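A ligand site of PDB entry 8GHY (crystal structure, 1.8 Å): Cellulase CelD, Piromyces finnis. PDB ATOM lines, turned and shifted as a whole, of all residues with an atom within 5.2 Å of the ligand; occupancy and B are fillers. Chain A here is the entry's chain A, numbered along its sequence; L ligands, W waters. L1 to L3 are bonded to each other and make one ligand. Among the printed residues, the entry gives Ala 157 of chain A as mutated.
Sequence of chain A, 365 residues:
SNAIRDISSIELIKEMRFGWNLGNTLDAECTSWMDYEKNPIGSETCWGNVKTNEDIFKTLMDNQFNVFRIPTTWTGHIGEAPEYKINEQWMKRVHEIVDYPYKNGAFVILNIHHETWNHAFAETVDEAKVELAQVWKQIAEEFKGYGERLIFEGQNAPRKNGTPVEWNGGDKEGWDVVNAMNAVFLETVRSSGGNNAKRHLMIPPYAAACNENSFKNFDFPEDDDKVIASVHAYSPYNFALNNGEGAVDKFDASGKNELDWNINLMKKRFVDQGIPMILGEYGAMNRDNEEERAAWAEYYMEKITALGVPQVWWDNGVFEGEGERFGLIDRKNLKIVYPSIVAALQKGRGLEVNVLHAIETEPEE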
ATOM      1  N   ASN A  24       8.039 -29.736  25.609  1.00  0.00           N
ATOM      2  CA  ASN A  24       7.400 -30.717  24.706  1.00  0.00           C
ATOM      3  C   ASN A  24       7.750 -32.145  25.102  1.00  0.00           C
ATOM      4  O   ASN A  24       7.988 -33.004  24.247  1.00  0.00           O
ATOM      5  CB  ASN A  24       7.773 -30.441  23.255  1.00  0.00           C
ATOM      6  CG  ASN A  24       6.934 -29.348  22.640  1.00  0.00           C
ATOM      7  OD1 ASN A  24       6.310 -28.564  23.345  1.00  0.00           O
ATOM      8  ND2 ASN A  24       6.921 -29.276  21.294  1.00  0.00           N
ATOM      9  N   ASP A  27       5.129 -32.393  29.268  1.00  0.00           N
ATOM     10  CA  ASP A  27       3.998 -31.540  28.969  1.00  0.00           C
ATOM     11  C   ASP A  27       3.269 -31.949  27.699  1.00  0.00           C
ATOM     12  O   ASP A  27       2.197 -31.419  27.422  1.00  0.00           O
ATOM     13  CB  ASP A  27       4.453 -30.074  28.837  1.00  0.00           C
ATOM     14  CG  ASP A  27       5.718 -29.910  28.004  1.00  0.00           C
ATOM     15  OD1 ASP A  27       6.682 -30.693  28.206  1.00  0.00           O
ATOM     16  OD2 ASP A  27       5.750 -29.005  27.135  1.00  0.00           O
ATOM     17  N   TRP A  47       5.433 -36.262  21.486  1.00  0.00           N
ATOM     18  CA  TRP A  47       5.670 -35.122  20.606  1.00  0.00           C
ATOM     19  C   TRP A  47       7.059 -35.176  19.981  1.00  0.00           C
ATOM     20  O   TRP A  47       7.551 -34.144  19.508  1.00  0.00           O
ATOM     21  CB  TRP A  47       5.440 -33.803  21.360  1.00  0.00           C
ATOM     22  CG  TRP A  47       3.978 -33.469  21.560  1.00  0.00           C
ATOM     23  CD1 TRP A  47       2.903 -34.212  21.141  1.00  0.00           C
ATOM     24  CD2 TRP A  47       3.430 -32.308  22.207  1.00  0.00           C
ATOM     25  NE1 TRP A  47       1.724 -33.592  21.502  1.00  0.00           N
ATOM     26  CE2 TRP A  47       2.026 -32.420  22.149  1.00  0.00           C
ATOM     27  CE3 TRP A  47       3.991 -31.191  22.832  1.00  0.00           C
ATOM     28  CZ2 TRP A  47       1.172 -31.457  22.704  1.00  0.00           C
ATOM     29  CZ3 TRP A  47       3.137 -30.228  23.387  1.00  0.00           C
ATOM     30  CH2 TRP A  47       1.746 -30.365  23.311  1.00  0.00           C
ATOM     31  N   ARG A  69      13.471 -26.452  34.560  1.00  0.00           N
ATOM     32  CA  ARG A  69      12.018 -26.486  34.685  1.00  0.00           C
ATOM     33  C   ARG A  69      11.513 -27.721  33.964  1.00  0.00           C
ATOM     34  O   ARG A  69      11.944 -28.012  32.846  1.00  0.00           O
ATOM     35  CB  ARG A  69      11.384 -25.218  34.116  1.00  0.00           C
ATOM     36  CG  ARG A  69       9.873 -25.105  34.349  1.00  0.00           C
ATOM     37  CD  ARG A  69       9.454 -23.650  34.139  1.00  0.00           C
ATOM     38  NE  ARG A  69       8.018 -23.426  34.131  1.00  0.00           N
ATOM     39  CZ  ARG A  69       7.279 -23.363  33.034  1.00  0.00           C
ATOM     40  NH1 ARG A  69       7.782 -23.648  31.841  1.00  0.00           N
ATOM     41  NH2 ARG A  69       5.996 -22.987  33.128  1.00  0.00           N
ATOM     42  N   HIS A 113       0.938 -28.088  33.688  1.00  0.00           N
ATOM     43  CA  HIS A 113       1.137 -27.416  32.403  1.00  0.00           C
ATOM     44  C   HIS A 113      -0.098 -27.372  31.505  1.00  0.00           C
ATOM     45  O   HIS A 113      -1.001 -26.566  31.744  1.00  0.00           O
ATOM     46  CB  HIS A 113       2.311 -28.063  31.661  1.00  0.00           C
ATOM     47  CG  HIS A 113       3.097 -27.097  30.812  1.00  0.00           C
ATOM     48  ND1 HIS A 113       4.010 -26.218  31.358  1.00  0.00           N
ATOM     49  CD2 HIS A 113       3.092 -26.866  29.478  1.00  0.00           C
ATOM     50  CE1 HIS A 113       4.546 -25.489  30.381  1.00  0.00           C
ATOM     51  NE2 HIS A 113       3.997 -25.858  29.233  1.00  0.00           N
ATOM     52  N   HIS A 114      -0.138 -28.171  30.431  1.00  0.00           N
ATOM     53  CA  HIS A 114      -1.186 -28.064  29.408  1.00  0.00           C
ATOM     54  C   HIS A 114      -2.487 -28.740  29.859  1.00  0.00           C
ATOM     55  O   HIS A 114      -3.023 -29.628  29.197  1.00  0.00           O
ATOM     56  CB  HIS A 114      -0.723 -28.665  28.086  1.00  0.00           C
ATOM     57  CG  HIS A 114       0.291 -27.844  27.355  1.00  0.00           C
ATOM     58  ND1 HIS A 114       0.267 -26.464  27.327  1.00  0.00           N
ATOM     59  CD2 HIS A 114       1.361 -28.208  26.611  1.00  0.00           C
ATOM     60  CE1 HIS A 114       1.279 -26.019  26.607  1.00  0.00           C
ATOM     61  NE2 HIS A 114       1.961 -27.059  26.167  1.00  0.00           N
ATOM     62  N   ASN A 156       0.593 -23.063  35.006  1.00  0.00           N
ATOM     63  CA  ASN A 156       1.509 -22.616  33.964  1.00  0.00           C
ATOM     64  C   ASN A 156       1.071 -21.285  33.376  1.00  0.00           C
ATOM     65  O   ASN A 156       1.622 -20.237  33.700  1.00  0.00           O
ATOM     66  CB  ASN A 156       1.604 -23.670  32.858  1.00  0.00           C
ATOM     67  CG  ASN A 156       2.463 -23.201  31.708  1.00  0.00           C
ATOM     68  OD1 ASN A 156       3.545 -22.647  31.911  1.00  0.00           O
ATOM     69  ND2 ASN A 156       1.974 -23.400  30.485  1.00  0.00           N
ATOM     70  N   ALA A 157       0.076 -21.321  32.482  1.00  0.00           N
ATOM     71  CA  ALA A 157      -0.460 -20.118  31.863  1.00  0.00           C
ATOM     72  C   ALA A 157      -1.981 -20.189  31.866  1.00  0.00           C
ATOM     73  O   ALA A 157      -2.624 -20.180  30.814  1.00  0.00           O
ATOM     74  CB  ALA A 157       0.081 -19.950  30.438  1.00  0.00           C
ATOM     75  N   TRP A 167      -4.849 -14.124  24.841  1.00  0.00           N
ATOM     76  CA  TRP A 167      -3.451 -13.767  24.659  1.00  0.00           C
ATOM     77  C   TRP A 167      -3.197 -12.258  24.715  1.00  0.00           C
ATOM     78  O   TRP A 167      -2.165 -11.792  24.225  1.00  0.00           O
ATOM     79  CB  TRP A 167      -2.918 -14.325  23.331  1.00  0.00           C
ATOM     80  CG  TRP A 167      -2.887 -15.819  23.295  1.00  0.00           C
ATOM     81  CD1 TRP A 167      -3.526 -16.633  22.383  1.00  0.00           C
ATOM     82  CD2 TRP A 167      -2.197 -16.689  24.203  1.00  0.00           C
ATOM     83  NE1 TRP A 167      -3.255 -17.949  22.676  1.00  0.00           N
ATOM     84  CE2 TRP A 167      -2.458 -18.014  23.784  1.00  0.00           C
ATOM     85  CE3 TRP A 167      -1.398 -16.477  25.323  1.00  0.00           C
ATOM     86  CZ2 TRP A 167      -1.927 -19.118  24.451  1.00  0.00           C
ATOM     87  CZ3 TRP A 167      -0.873 -17.575  25.984  1.00  0.00           C
ATOM     88  CH2 TRP A 167      -1.143 -18.876  25.547  1.00  0.00           C
ATOM     89  N   HIS A 232       6.270 -15.323  31.843  1.00  0.00           N
ATOM     90  CA  HIS A 232       6.835 -15.775  30.569  1.00  0.00           C
ATOM     91  C   HIS A 232       6.934 -14.556  29.657  1.00  0.00           C
ATOM     92  O   HIS A 232       6.057 -13.688  29.652  1.00  0.00           O
ATOM     93  CB  HIS A 232       5.966 -16.872  29.943  1.00  0.00           C
ATOM     94  CG  HIS A 232       5.801 -18.081  30.825  1.00  0.00           C
ATOM     95  ND1 HIS A 232       4.918 -19.103  30.545  1.00  0.00           N
ATOM     96  CD2 HIS A 232       6.408 -18.426  31.988  1.00  0.00           C
ATOM     97  CE1 HIS A 232       4.983 -20.024  31.491  1.00  0.00           C
ATOM     98  NE2 HIS A 232       5.877 -19.638  32.377  1.00  0.00           N
ATOM     99  N   TYR A 234       8.462 -13.954  25.885  1.00  0.00           N
ATOM    100  CA  TYR A 234       9.093 -14.189  24.591  1.00  0.00           C
ATOM    101  C   TYR A 234       9.063 -12.882  23.812  1.00  0.00           C
ATOM    102  O   TYR A 234       8.212 -12.640  22.950  1.00  0.00           O
ATOM    103  CB  TYR A 234       8.364 -15.288  23.821  1.00  0.00           C
ATOM    104  CG  TYR A 234       8.338 -16.659  24.461  1.00  0.00           C
ATOM    105  CD1 TYR A 234       7.496 -16.943  25.539  1.00  0.00           C
ATOM    106  CD2 TYR A 234       9.098 -17.684  23.932  1.00  0.00           C
ATOM    107  CE1 TYR A 234       7.452 -18.221  26.084  1.00  0.00           C
ATOM    108  CE2 TYR A 234       9.067 -18.946  24.464  1.00  0.00           C
ATOM    109  CZ  TYR A 234       8.239 -19.216  25.544  1.00  0.00           C
ATOM    110  OH  TYR A 234       8.211 -20.493  26.059  1.00  0.00           O
ATOM    111  N   LEU A 241       8.791 -15.147  18.903  1.00  0.00           N
ATOM    112  CA  LEU A 241       7.743 -16.136  19.079  1.00  0.00           C
ATOM    113  C   LEU A 241       6.798 -16.270  17.885  1.00  0.00           C
ATOM    114  O   LEU A 241       6.267 -17.359  17.668  1.00  0.00           O
ATOM    115  CB  LEU A 241       6.901 -15.803  20.327  1.00  0.00           C
ATOM    116  CG  LEU A 241       5.745 -16.728  20.711  1.00  0.00           C
ATOM    117  CD1 LEU A 241       6.208 -18.155  20.907  1.00  0.00           C
ATOM    118  CD2 LEU A 241       5.049 -16.204  21.973  1.00  0.00           C
ATOM    119  N   GLU A 281       9.852 -18.982  31.342  1.00  0.00           N
ATOM    120  CA  GLU A 281       9.920 -19.320  29.934  1.00  0.00           C
ATOM    121  C   GLU A 281      10.277 -18.080  29.137  1.00  0.00           C
ATOM    122  O   GLU A 281       9.726 -17.001  29.381  1.00  0.00           O
ATOM    123  CB  GLU A 281       8.601 -19.859  29.382  1.00  0.00           C
ATOM    124  CG  GLU A 281       8.140 -21.165  29.949  1.00  0.00           C
ATOM    125  CD  GLU A 281       6.924 -21.666  29.210  1.00  0.00           C
ATOM    126  OE1 GLU A 281       6.706 -21.225  28.050  1.00  0.00           O
ATOM    127  OE2 GLU A 281       6.193 -22.500  29.772  1.00  0.00           O
ATOM    128  N   TRP A 314      13.175 -21.736  26.993  1.00  0.00           N
ATOM    129  CA  TRP A 314      12.195 -22.739  26.572  1.00  0.00           C
ATOM    130  C   TRP A 314      12.781 -23.540  25.410  1.00  0.00           C
ATOM    131  O   TRP A 314      13.004 -23.002  24.321  1.00  0.00           O
ATOM    132  CB  TRP A 314      10.885 -22.080  26.153  1.00  0.00           C
ATOM    133  CG  TRP A 314       9.897 -23.082  25.625  1.00  0.00           C
ATOM    134  CD1 TRP A 314       9.575 -23.298  24.319  1.00  0.00           C
ATOM    135  CD2 TRP A 314       9.117 -24.006  26.393  1.00  0.00           C
ATOM    136  NE1 TRP A 314       8.644 -24.299  24.215  1.00  0.00           N
ATOM    137  CE2 TRP A 314       8.336 -24.752  25.477  1.00  0.00           C
ATOM    138  CE3 TRP A 314       8.984 -24.273  27.753  1.00  0.00           C
ATOM    139  CZ2 TRP A 314       7.451 -25.747  25.879  1.00  0.00           C
ATOM    140  CZ3 TRP A 314       8.095 -25.264  28.162  1.00  0.00           C
ATOM    141  CH2 TRP A 314       7.349 -26.000  27.224  1.00  0.00           C
ATOM    142  N   ASN A 316      11.893 -26.782  23.266  1.00  0.00           N
ATOM    143  CA  ASN A 316      10.906 -27.797  22.922  1.00  0.00           C
ATOM    144  C   ASN A 316      11.479 -28.896  22.017  1.00  0.00           C
ATOM    145  O   ASN A 316      10.728 -29.756  21.556  1.00  0.00           O
ATOM    146  CB  ASN A 316       9.691 -27.158  22.252  1.00  0.00           C
ATOM    147  CG  ASN A 316       9.997 -26.517  20.907  1.00  0.00           C
ATOM    148  OD1 ASN A 316      11.166 -26.372  20.519  1.00  0.00           O
ATOM    149  ND2 ASN A 316       8.959 -26.118  20.197  1.00  0.00           N
ATOM    150  N   VAL A 318      12.600 -28.716  19.017  1.00  0.00           N
ATOM    151  CA  VAL A 318      12.296 -28.524  17.603  1.00  0.00           C
ATOM    152  C   VAL A 318      13.305 -27.568  17.004  1.00  0.00           C
ATOM    153  O   VAL A 318      13.534 -26.470  17.532  1.00  0.00           O
ATOM    154  CB  VAL A 318      10.861 -27.997  17.418  1.00  0.00           C
ATOM    155  CG1 VAL A 318      10.520 -27.890  15.925  1.00  0.00           C
ATOM    156  CG2 VAL A 318       9.870 -28.895  18.138  1.00  0.00           C
ATOM    157  N   GLU A 324       7.212 -24.466  16.187  1.00  0.00           N
ATOM    158  CA  GLU A 324       8.029 -23.476  16.874  1.00  0.00           C
ATOM    159  C   GLU A 324       9.408 -24.067  17.147  1.00  0.00           C
ATOM    160  O   GLU A 324       9.514 -25.131  17.759  1.00  0.00           O
ATOM    161  CB  GLU A 324       7.335 -23.039  18.168  1.00  0.00           C
ATOM    162  CG  GLU A 324       5.898 -22.564  17.970  1.00  0.00           C
ATOM    163  CD  GLU A 324       5.258 -22.025  19.245  1.00  0.00           C
ATOM    164  OE1 GLU A 324       5.826 -22.243  20.334  1.00  0.00           O
ATOM    165  OE2 GLU A 324       4.195 -21.376  19.154  1.00  0.00           O
ATOM    166  N   PHE A 326      12.418 -23.844  18.964  1.00  0.00           N
ATOM    167  CA  PHE A 326      13.102 -23.344  20.162  1.00  0.00           C
ATOM    168  C   PHE A 326      14.207 -24.269  20.646  1.00  0.00           C
ATOM    169  O   PHE A 326      14.740 -24.062  21.739  1.00  0.00           O
ATOM    170  CB  PHE A 326      12.090 -23.104  21.294  1.00  0.00           C
ATOM    171  CG  PHE A 326      11.217 -21.906  21.087  1.00  0.00           C
ATOM    172  CD1 PHE A 326      11.743 -20.622  21.164  1.00  0.00           C
ATOM    173  CD2 PHE A 326       9.855 -22.048  20.866  1.00  0.00           C
ATOM    174  CE1 PHE A 326      10.936 -19.504  20.986  1.00  0.00           C
ATOM    175  CE2 PHE A 326       9.046 -20.942  20.679  1.00  0.00           C
ATOM    176  CZ  PHE A 326       9.577 -19.661  20.748  1.00  0.00           C
HETATM  177  C1  LIG L   1       3.681 -22.493  27.069  1.00  0.00           C
HETATM  178  C2  LIG L   1       4.616 -23.452  26.331  1.00  0.00           C
HETATM  179  C3  LIG L   1       4.665 -23.055  24.857  1.00  0.00           C
HETATM  180  C4  LIG L   1       5.209 -21.626  24.807  1.00  0.00           C
HETATM  181  C5  LIG L   1       5.622 -21.155  23.420  1.00  0.00           C
HETATM  182  C6  LIG L   1       3.947 -21.013  26.743  1.00  0.00           C
HETATM  183  O1  LIG L   1       2.789 -20.276  27.145  1.00  0.00           O
HETATM  184  O2  LIG L   1       3.826 -22.697  28.484  1.00  0.00           O
HETATM  185  O3  LIG L   1       4.106 -24.781  26.476  1.00  0.00           O
HETATM  186  O4  LIG L   1       5.493 -23.952  24.126  1.00  0.00           O
HETATM  187  O5  LIG L   1       4.177 -20.783  25.344  1.00  0.00           O
HETATM  188  O6  LIG L   1       4.465 -21.119  22.559  1.00  0.00           O
HETATM  189  C1  LG2 L   2       5.853 -25.219  22.107  1.00  0.00           C
HETATM  190  C2  LG2 L   2       5.145 -25.733  20.851  1.00  0.00           C
HETATM  191  C3  LG2 L   2       3.864 -26.494  21.205  1.00  0.00           C
HETATM  192  C4  LG2 L   2       3.003 -25.678  22.185  1.00  0.00           C
HETATM  193  C5  LG2 L   2       1.772 -26.426  22.688  1.00  0.00           C
HETATM  194  C6  LG2 L   2       4.853 -24.440  22.948  1.00  0.00           C
HETATM  195  O1  LG2 L   2       6.952 -24.378  21.745  1.00  0.00           O
HETATM  196  O2  LG2 L   2       6.027 -26.571  20.110  1.00  0.00           O
HETATM  197  O3  LG2 L   2       3.126 -26.689  19.998  1.00  0.00           O
HETATM  198  O4  LG2 L   2       3.792 -25.304  23.319  1.00  0.00           O
HETATM  199  O5  LG2 L   2       0.836 -25.512  23.270  1.00  0.00           O
HETATM  200  C1  LG3 L   3       1.403 -27.856  18.844  1.00  0.00           C
HETATM  201  C2  LG3 L   3       0.816 -29.220  18.519  1.00  0.00           C
HETATM  202  C3  LG3 L   3       1.910 -30.203  18.140  1.00  0.00           C
HETATM  203  C4  LG3 L   3       3.034 -30.189  19.159  1.00  0.00           C
HETATM  204  C5  LG3 L   3       4.155 -31.142  18.767  1.00  0.00           C
HETATM  205  C6  LG3 L   3       2.573 -27.983  19.822  1.00  0.00           C
HETATM  206  O1  LG3 L   3       0.391 -27.006  19.402  1.00  0.00           O
HETATM  207  O2  LG3 L   3      -0.121 -29.091  17.449  1.00  0.00           O
HETATM  208  O3  LG3 L   3       1.352 -31.530  18.117  1.00  0.00           O
HETATM  209  O4  LG3 L   3       3.559 -28.866  19.304  1.00  0.00           O
HETATM  210  O5  LG3 L   3       4.907 -30.562  17.702  1.00  0.00           O
HETATM  211  O   HOH W   1       3.012 -18.242  24.527  1.00  0.00           O
HETATM  212  O   HOH W   2       3.037 -24.906  17.097  1.00  0.00           O
HETATM  213  O   HOH W   3       0.376 -22.058  26.870  1.00  0.00           O
HETATM  214  O   HOH W   4       0.568 -22.906  24.364  1.00  0.00           O
HETATM  215  O   HOH W   5       2.902 -18.394  28.726  1.00  0.00           O
HETATM  216  O   HOH W   6       5.371 -26.493  17.561  1.00  0.00           O
HETATM  217  O   HOH W   7       1.993 -22.352  20.493  1.00  0.00           O
HETATM  218  O   HOH W   8       1.944 -21.108  22.947  1.00  0.00           O
HETATM  219  O   HOH W   9       4.587 -27.470  25.424  1.00  0.00           O
HETATM  220  O   HOH W  10      -1.254 -27.175  24.062  1.00  0.00           O
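The side-chain amide nitrogen of Asn 156 sits at hydrogen-bond distance from an oxygen (O2) of LIG L1, 2.8 Å away.
OE2 of Glu 281 sits at hydrogen-bond distance from O2 of LIG L1, 2.7 Å away.
An oxygen (O3) of LIG L1 lies close to a ring nitrogen (NE2) of His 114 (3.1 Å).
The side-chain amide nitrogen (ND2) of Asn 316 is in hydrogen-bond range of an oxygen (O2) of LG2 L2 (3.0 Å).
The side-chain carboxylate (OE1) of Glu 324 is in hydrogen-bond range of an oxygen (O1) of LG2 L2 (2.8 Å).
ND2 of Asn 24 lies within hydrogen-bond range of O2 of LG2 L2 (3.1 Å).
NE2 of His 113 is in hydrogen-bond range of O3 of LIG L1 (3.0 Å).
The indole nitrogen (NE1) of Trp 314 is in hydrogen-bond range of an oxygen (O1) of LG2 L2.
N of Phe 326 lies within hydrogen-bond range of OD1 of Asn 316.
O of Glu 324 lies within hydrogen-bond range of ND2 of Asn 316 (2.7 Å).
The side-chain carboxylate of Glu 281 lies close to the side-chain amide oxygen of Asn 156.
The side-chain amide oxygen (OD1) of Asn 316 sits at hydrogen-bond distance from the backbone NH (N) of Val 318 (3.1 Å).
The side-chain carboxylate (OE2) of Glu 281 is in salt-bridge range of the guanidinium group (NH1) of Arg 69 (2.9 Å).
OD2 of Asp 27 is in hydrogen-bond range of N of Asn 24, at 2.8 Å.
The side-chain amide nitrogen (ND2) of Asn 156 sits close to a ring nitrogen (NE2) of His 113.
OE1 of Glu 281 sits at hydrogen-bond distance from OH of Tyr 234 (2.6 Å).
Merely in contact with the ligand: Tyr 234 (3.4 Å), Trp 47 (3.6 Å), Leu 241 (3.8 Å) and Phe 326 (3.8 Å).
Hydrophobic or aromatic side chains that line the ligand: Trp 47, His 113, His 114, Tyr 234, Leu 241, Trp 314 and Phe 326.
12 residues have an atom within 4 Å of the ligand: Asn 24, Trp 47, His 113, His 114, Asn 156, Tyr 234, Leu 241, Glu 281, Trp 314, Asn 316, Glu 324 and Phe 326.
Water W5 bridges an oxygen (O1) of LIG L1 and a ring nitrogen (ND1) of His 232.
Water W6 lies within hydrogen-bond range of O2 of LG2 L2 (2.6 Å) and N of Glu 324 (3.1 Å).
Water W9 lies within hydrogen-bond range of the side-chain carboxylate (OD2) of Asp 27 (2.6 Å), a ring nitrogen (NE2) of His 114 (2.8 Å), the side-chain amide oxygen (OD1) of Asn 24 (2.9 Å) and an oxygen (O3) of LIG L1 (2.9 Å).
Water W7 lies within hydrogen-bond range of OE2 of Glu 324 (2.8 Å) and O6 of LIG L1 (3.4 Å).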
